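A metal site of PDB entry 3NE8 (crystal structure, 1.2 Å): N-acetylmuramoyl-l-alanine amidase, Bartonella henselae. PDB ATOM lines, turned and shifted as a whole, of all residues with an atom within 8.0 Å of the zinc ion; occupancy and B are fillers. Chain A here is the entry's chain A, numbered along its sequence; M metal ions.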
ATOM      1  N   PRO A  11      15.704  14.739 -31.404  1.00  0.00           N
ATOM      2  CA  PRO A  11      15.623  16.201 -31.364  1.00  0.00           C
ATOM      3  C   PRO A  11      15.052  16.641 -30.019  1.00  0.00           C
ATOM      4  O   PRO A  11      13.884  16.361 -29.707  1.00  0.00           O
ATOM      5  CB  PRO A  11      14.660  16.550 -32.509  1.00  0.00           C
ATOM      6  CG  PRO A  11      14.498  15.280 -33.313  1.00  0.00           C
ATOM      7  CD  PRO A  11      14.729  14.154 -32.345  1.00  0.00           C
ATOM      8  N   GLY A  12      15.868  17.304 -29.198  1.00  0.00           N
ATOM      9  CA  GLY A  12      15.424  17.697 -27.872  1.00  0.00           C
ATOM     10  C   GLY A  12      14.141  18.510 -27.881  1.00  0.00           C
ATOM     11  O   GLY A  12      13.880  19.286 -28.803  1.00  0.00           O
ATOM     12  N   HIS A  13      13.342  18.321 -26.830  1.00  0.00           N
ATOM     13  CA  HIS A  13      12.124  19.105 -26.609  1.00  0.00           C
ATOM     14  C   HIS A  13      11.086  18.781 -27.664  1.00  0.00           C
ATOM     15  O   HIS A  13      11.138  17.684 -28.234  1.00  0.00           O
ATOM     16  CB  HIS A  13      12.457  20.595 -26.452  1.00  0.00           C
ATOM     17  CG  HIS A  13      13.608  20.794 -25.514  1.00  0.00           C
ATOM     18  ND1 HIS A  13      13.480  20.721 -24.147  1.00  0.00           N
ATOM     19  CD2 HIS A  13      14.932  20.908 -25.766  1.00  0.00           C
ATOM     20  CE1 HIS A  13      14.673  20.828 -23.590  1.00  0.00           C
ATOM     21  NE2 HIS A  13      15.576  20.939 -24.552  1.00  0.00           N
ATOM     22  N   ASP A  17       6.807  21.792 -25.045  1.00  0.00           N
ATOM     23  CA  ASP A  17       8.133  22.162 -24.551  1.00  0.00           C
ATOM     24  C   ASP A  17       8.941  22.817 -25.682  1.00  0.00           C
ATOM     25  O   ASP A  17       9.507  22.129 -26.546  1.00  0.00           O
ATOM     26  CB  ASP A  17       8.869  20.920 -24.024  1.00  0.00           C
ATOM     27  CG  ASP A  17      10.262  21.223 -23.516  1.00  0.00           C
ATOM     28  OD1 ASP A  17      10.627  22.413 -23.401  1.00  0.00           O
ATOM     29  OD2 ASP A  17      10.990  20.263 -23.194  1.00  0.00           O
ATOM     30  N   GLY A  18       8.996  24.139 -25.681  1.00  0.00           N
ATOM     31  CA  GLY A  18       9.756  24.841 -26.701  1.00  0.00           C
ATOM     32  C   GLY A  18      11.259  24.801 -26.482  1.00  0.00           C
ATOM     33  O   GLY A  18      12.032  25.107 -27.386  1.00  0.00           O
ATOM     34  N   GLY A  19      11.689  24.427 -25.277  1.00  0.00           N
ATOM     35  CA  GLY A  19      13.092  24.527 -24.912  1.00  0.00           C
ATOM     36  C   GLY A  19      13.538  25.985 -24.806  1.00  0.00           C
ATOM     37  O   GLY A  19      12.722  26.882 -24.596  1.00  0.00           O
ATOM     38  N   ALA A  20      14.836  26.216 -24.950  1.00  0.00           N
ATOM     39  CA  ALA A  20      15.392  27.570 -24.841  1.00  0.00           C
ATOM     40  C   ALA A  20      14.889  28.459 -25.969  1.00  0.00           C
ATOM     41  O   ALA A  20      14.512  27.990 -27.039  1.00  0.00           O
ATOM     42  CB  ALA A  20      16.908  27.504 -24.850  1.00  0.00           C
ATOM     43  N   GLU A  28      14.584  26.375 -29.316  1.00  0.00           N
ATOM     44  CA  GLU A  28      15.388  25.172 -29.277  1.00  0.00           C
ATOM     45  C   GLU A  28      14.686  23.993 -29.950  1.00  0.00           C
ATOM     46  O   GLU A  28      15.305  23.269 -30.737  1.00  0.00           O
ATOM     47  CB  GLU A  28      15.759  24.826 -27.845  1.00  0.00           C
ATOM     48  CG  GLU A  28      16.630  23.592 -27.729  1.00  0.00           C
ATOM     49  CD  GLU A  28      16.984  23.250 -26.307  1.00  0.00           C
ATOM     50  OE1 GLU A  28      16.452  23.894 -25.376  1.00  0.00           O
ATOM     51  OE2 GLU A  28      17.786  22.315 -26.129  1.00  0.00           O
ATOM     52  N   LYS A  29      13.390  23.798 -29.684  1.00  0.00           N
ATOM     53  CA  LYS A  29      12.714  22.626 -30.230  1.00  0.00           C
ATOM     54  C   LYS A  29      12.724  22.627 -31.760  1.00  0.00           C
ATOM     55  O   LYS A  29      12.696  21.561 -32.383  1.00  0.00           O
ATOM     56  CB  LYS A  29      11.273  22.518 -29.720  1.00  0.00           C
ATOM     57  CG  LYS A  29      10.317  23.598 -30.208  1.00  0.00           C
ATOM     58  CD  LYS A  29       8.872  23.177 -29.977  1.00  0.00           C
ATOM     59  CE  LYS A  29       7.893  24.272 -30.373  1.00  0.00           C
ATOM     60  NZ  LYS A  29       6.483  23.771 -30.269  1.00  0.00           N
ATOM     61  N   THR A  32      16.594  21.958 -32.912  1.00  0.00           N
ATOM     62  CA  THR A  32      17.053  20.579 -32.742  1.00  0.00           C
ATOM     63  C   THR A  32      16.440  19.657 -33.809  1.00  0.00           C
ATOM     64  O   THR A  32      17.116  18.759 -34.299  1.00  0.00           O
ATOM     65  CB  THR A  32      16.738  20.026 -31.345  1.00  0.00           C
ATOM     66  OG1 THR A  32      15.307  19.995 -31.176  1.00  0.00           O
ATOM     67  CG2 THR A  32      17.409  20.868 -30.255  1.00  0.00           C
ATOM     68  N   SER A  80      21.211  12.589 -28.581  1.00  0.00           N
ATOM     69  CA  SER A  80      20.209  13.588 -28.238  1.00  0.00           C
ATOM     70  C   SER A  80      20.770  14.959 -28.555  1.00  0.00           C
ATOM     71  O   SER A  80      21.892  15.301 -28.132  1.00  0.00           O
ATOM     72  CB  SER A  80      19.828  13.484 -26.769  1.00  0.00           C
ATOM     73  OG  SER A  80      18.712  14.308 -26.459  1.00  0.00           O
ATOM     74  N   ILE A  81      19.998  15.747 -29.291  1.00  0.00           N
ATOM     75  CA  ILE A  81      20.450  17.006 -29.871  1.00  0.00           C
ATOM     76  C   ILE A  81      19.780  18.181 -29.166  1.00  0.00           C
ATOM     77  O   ILE A  81      18.543  18.228 -29.074  1.00  0.00           O
ATOM     78  CB  ILE A  81      20.095  17.030 -31.369  1.00  0.00           C
ATOM     79  CG1 ILE A  81      20.826  15.912 -32.114  1.00  0.00           C
ATOM     80  CG2 ILE A  81      20.370  18.405 -31.998  1.00  0.00           C
ATOM     81  CD1 ILE A  81      20.193  15.481 -33.405  1.00  0.00           C
ATOM     82  N   HIS A  82      20.592  19.118 -28.667  1.00  0.00           N
ATOM     83  CA  HIS A  82      20.143  20.231 -27.840  1.00  0.00           C
ATOM     84  C   HIS A  82      20.787  21.546 -28.207  1.00  0.00           C
ATOM     85  O   HIS A  82      21.815  21.573 -28.883  1.00  0.00           O
ATOM     86  CB  HIS A  82      20.390  19.905 -26.364  1.00  0.00           C
ATOM     87  CG  HIS A  82      19.460  18.858 -25.853  1.00  0.00           C
ATOM     88  ND1 HIS A  82      18.301  19.178 -25.166  1.00  0.00           N
ATOM     89  CD2 HIS A  82      19.442  17.516 -26.036  1.00  0.00           C
ATOM     90  CE1 HIS A  82      17.627  18.066 -24.918  1.00  0.00           C
ATOM     91  NE2 HIS A  82      18.298  17.050 -25.437  1.00  0.00           N
ATOM     92  N   ALA A  83      20.156  22.637 -27.764  1.00  0.00           N
ATOM     93  CA  ALA A  83      20.706  23.977 -27.884  1.00  0.00           C
ATOM     94  C   ALA A  83      20.176  24.802 -26.716  1.00  0.00           C
ATOM     95  O   ALA A  83      19.298  25.655 -26.864  1.00  0.00           O
ATOM     96  CB  ALA A  83      20.321  24.598 -29.216  1.00  0.00           C
ATOM     97  N   ASP A  84      20.701  24.519 -25.530  1.00  0.00           N
ATOM     98  CA  ASP A  84      20.114  24.990 -24.291  1.00  0.00           C
ATOM     99  C   ASP A  84      20.589  26.348 -23.839  1.00  0.00           C
ATOM    100  O   ASP A  84      21.524  26.931 -24.383  1.00  0.00           O
ATOM    101  CB  ASP A  84      20.405  23.973 -23.184  1.00  0.00           C
ATOM    102  CG  ASP A  84      19.581  22.720 -23.353  1.00  0.00           C
ATOM    103  OD1 ASP A  84      18.342  22.822 -23.230  1.00  0.00           O
ATOM    104  OD2 ASP A  84      20.148  21.644 -23.629  1.00  0.00           O
ATOM    105  N   THR A  85      19.908  26.868 -22.830  1.00  0.00           N
ATOM    106  CA  THR A  85      20.403  28.024 -22.093  1.00  0.00           C
ATOM    107  C   THR A  85      21.183  27.497 -20.897  1.00  0.00           C
ATOM    108  O   THR A  85      20.723  26.590 -20.206  1.00  0.00           O
ATOM    109  CB  THR A  85      19.247  28.906 -21.594  1.00  0.00           C
ATOM    110  OG1 THR A  85      18.734  29.676 -22.680  1.00  0.00           O
ATOM    111  CG2 THR A  85      19.716  29.841 -20.494  1.00  0.00           C
ATOM    112  N   LEU A 111      22.855  21.999 -15.797  1.00  0.00           N
ATOM    113  CA  LEU A 111      22.219  21.735 -17.081  1.00  0.00           C
ATOM    114  C   LEU A 111      21.404  20.438 -17.034  1.00  0.00           C
ATOM    115  O   LEU A 111      20.261  20.417 -17.490  1.00  0.00           O
ATOM    116  CB  LEU A 111      23.245  21.680 -18.202  1.00  0.00           C
ATOM    117  CG  LEU A 111      22.724  21.348 -19.602  1.00  0.00           C
ATOM    118  CD1 LEU A 111      21.716  22.382 -20.103  1.00  0.00           C
ATOM    119  CD2 LEU A 111      23.902  21.219 -20.567  1.00  0.00           C
ATOM    120  N   SER A 114      18.155  20.850 -15.007  1.00  0.00           N
ATOM    121  CA  SER A 114      17.132  21.562 -15.754  1.00  0.00           C
ATOM    122  C   SER A 114      16.566  20.734 -16.899  1.00  0.00           C
ATOM    123  O   SER A 114      15.349  20.722 -17.129  1.00  0.00           O
ATOM    124  CB  SER A 114      17.682  22.889 -16.287  1.00  0.00           C
ATOM    125  OG  SER A 114      17.944  23.786 -15.237  1.00  0.00           O
ATOM    126  N   GLU A 115      17.435  20.051 -17.628  1.00  0.00           N
ATOM    127  CA  GLU A 115      17.012  19.282 -18.790  1.00  0.00           C
ATOM    128  C   GLU A 115      16.200  18.046 -18.418  1.00  0.00           C
ATOM    129  O   GLU A 115      15.362  17.587 -19.201  1.00  0.00           O
ATOM    130  CB  GLU A 115      18.218  18.932 -19.661  1.00  0.00           C
ATOM    131  CG  GLU A 115      18.749  20.156 -20.383  1.00  0.00           C
ATOM    132  CD  GLU A 115      17.683  20.734 -21.268  1.00  0.00           C
ATOM    133  OE1 GLU A 115      17.031  21.743 -20.893  1.00  0.00           O
ATOM    134  OE2 GLU A 115      17.440  20.132 -22.329  1.00  0.00           O
ATOM    135  N   VAL A 118      12.179  18.833 -17.721  1.00  0.00           N
ATOM    136  CA  VAL A 118      11.222  19.149 -18.790  1.00  0.00           C
ATOM    137  C   VAL A 118      10.085  18.141 -18.927  1.00  0.00           C
ATOM    138  O   VAL A 118       9.017  18.485 -19.459  1.00  0.00           O
ATOM    139  CB  VAL A 118      11.898  19.368 -20.159  1.00  0.00           C
ATOM    140  CG1 VAL A 118      12.876  20.534 -20.077  1.00  0.00           C
ATOM    141  CG2 VAL A 118      12.566  18.098 -20.632  1.00  0.00           C
ATOM    142  N   PHE A 176      22.134  12.885 -16.992  1.00  0.00           N
ATOM    143  CA  PHE A 176      21.059  13.147 -17.957  1.00  0.00           C
ATOM    144  C   PHE A 176      20.178  11.906 -18.124  1.00  0.00           C
ATOM    145  O   PHE A 176      20.662  10.853 -18.560  1.00  0.00           O
ATOM    146  CB  PHE A 176      21.645  13.522 -19.319  1.00  0.00           C
ATOM    147  CG  PHE A 176      22.322  14.854 -19.353  1.00  0.00           C
ATOM    148  CD1 PHE A 176      21.602  16.003 -19.573  1.00  0.00           C
ATOM    149  CD2 PHE A 176      23.702  14.948 -19.186  1.00  0.00           C
ATOM    150  CE1 PHE A 176      22.234  17.244 -19.616  1.00  0.00           C
ATOM    151  CE2 PHE A 176      24.337  16.181 -19.236  1.00  0.00           C
ATOM    152  CZ  PHE A 176      23.612  17.324 -19.450  1.00  0.00           C
ATOM    153  N   LEU A 188      24.732  13.271 -25.533  1.00  0.00           N
ATOM    154  CA  LEU A 188      23.924  14.464 -25.720  1.00  0.00           C
ATOM    155  C   LEU A 188      24.835  15.537 -26.290  1.00  0.00           C
ATOM    156  O   LEU A 188      25.874  15.861 -25.703  1.00  0.00           O
ATOM    157  CB  LEU A 188      23.310  14.899 -24.383  1.00  0.00           C
ATOM    158  CG  LEU A 188      22.350  16.098 -24.420  1.00  0.00           C
ATOM    159  CD1 LEU A 188      21.323  15.978 -23.301  1.00  0.00           C
ATOM    160  CD2 LEU A 188      23.070  17.424 -24.366  1.00  0.00           C
ATOM    161  N   ILE A 189      24.483  16.063 -27.450  1.00  0.00           N
ATOM    162  CA  ILE A 189      25.294  17.087 -28.100  1.00  0.00           C
ATOM    163  C   ILE A 189      24.593  18.421 -28.024  1.00  0.00           C
ATOM    164  O   ILE A 189      23.452  18.552 -28.469  1.00  0.00           O
ATOM    165  CB  ILE A 189      25.580  16.744 -29.561  1.00  0.00           C
ATOM    166  CG1 ILE A 189      26.330  15.418 -29.658  1.00  0.00           C
ATOM    167  CG2 ILE A 189      26.382  17.860 -30.231  1.00  0.00           C
ATOM    168  CD1 ILE A 189      26.680  14.982 -31.068  1.00  0.00           C
ATOM    169  N   GLU A 190      25.263  19.397 -27.419  1.00  0.00           N
ATOM    170  CA  GLU A 190      24.816  20.777 -27.501  1.00  0.00           C
ATOM    171  C   GLU A 190      25.434  21.336 -28.763  1.00  0.00           C
ATOM    172  O   GLU A 190      26.663  21.445 -28.866  1.00  0.00           O
ATOM    173  CB  GLU A 190      25.275  21.598 -26.294  1.00  0.00           C
ATOM    174  CG  GLU A 190      24.662  21.162 -24.980  1.00  0.00           C
ATOM    175  CD  GLU A 190      23.210  21.572 -24.803  1.00  0.00           C
ATOM    176  OE1 GLU A 190      22.681  22.362 -25.615  1.00  0.00           O
ATOM    177  OE2 GLU A 190      22.598  21.089 -23.813  1.00  0.00           O
HETATM  178 ZN    ZN M   1      17.721  21.085 -24.292  1.00  0.00          ZN
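The side-chain carboxylate (OE1) of Glu 190 lies within hydrogen-bond range of the backbone NH (N) of Asp 84.
ND1 of His 13 is in hydrogen-bond range of OD2 of Asp 17, 2.7 Å away.
NE2 of His 82 is in hydrogen-bond range of OG of Ser 80, at 3.0 Å.
The backbone carbonyl oxygen (O) of Ile 189 lies within hydrogen-bond range of the backbone NH (N) of His 82, at 2.9 Å.
N of Ala 83 sits close to OE2 of Glu 28, at 2.9 Å.
The backbone NH (N) of Glu 28 is in hydrogen-bond range of the backbone carbonyl oxygen (O) of Ala 20 (2.8 Å).
The side-chain hydroxyl (OG1) of Thr 32 sits close to the backbone carbonyl oxygen (O) of Glu 28.
The backbone NH of Glu 28 sits at hydrogen-bond distance from the backbone carbonyl oxygen of Gly 18.
Within 4 Å of the zinc ion: His 13, Glu 28, His 82, Asp 84 and Glu 115.
The nearest printed residue that does not touch the zinc ion is Ala 83 (4.5 Å).
The side-chain carboxylate (OD1) of Asp 84 binds the zinc ion (2.1 Å).
The zinc ion is bound by a ring nitrogen (NE2) of His 13, 2.2 Å away.
ND1 of His 82 is bound to the zinc ion.
The zinc ion is bound by OE2 of Glu 115, 2.2 Å away.
OE2 of Glu 28 is bound to the zinc ion (2.2 Å).
OD2 of Asp 84 is bound to the zinc ion, 2.6 Å away.
The zinc ion has six donor atoms within binding distance.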
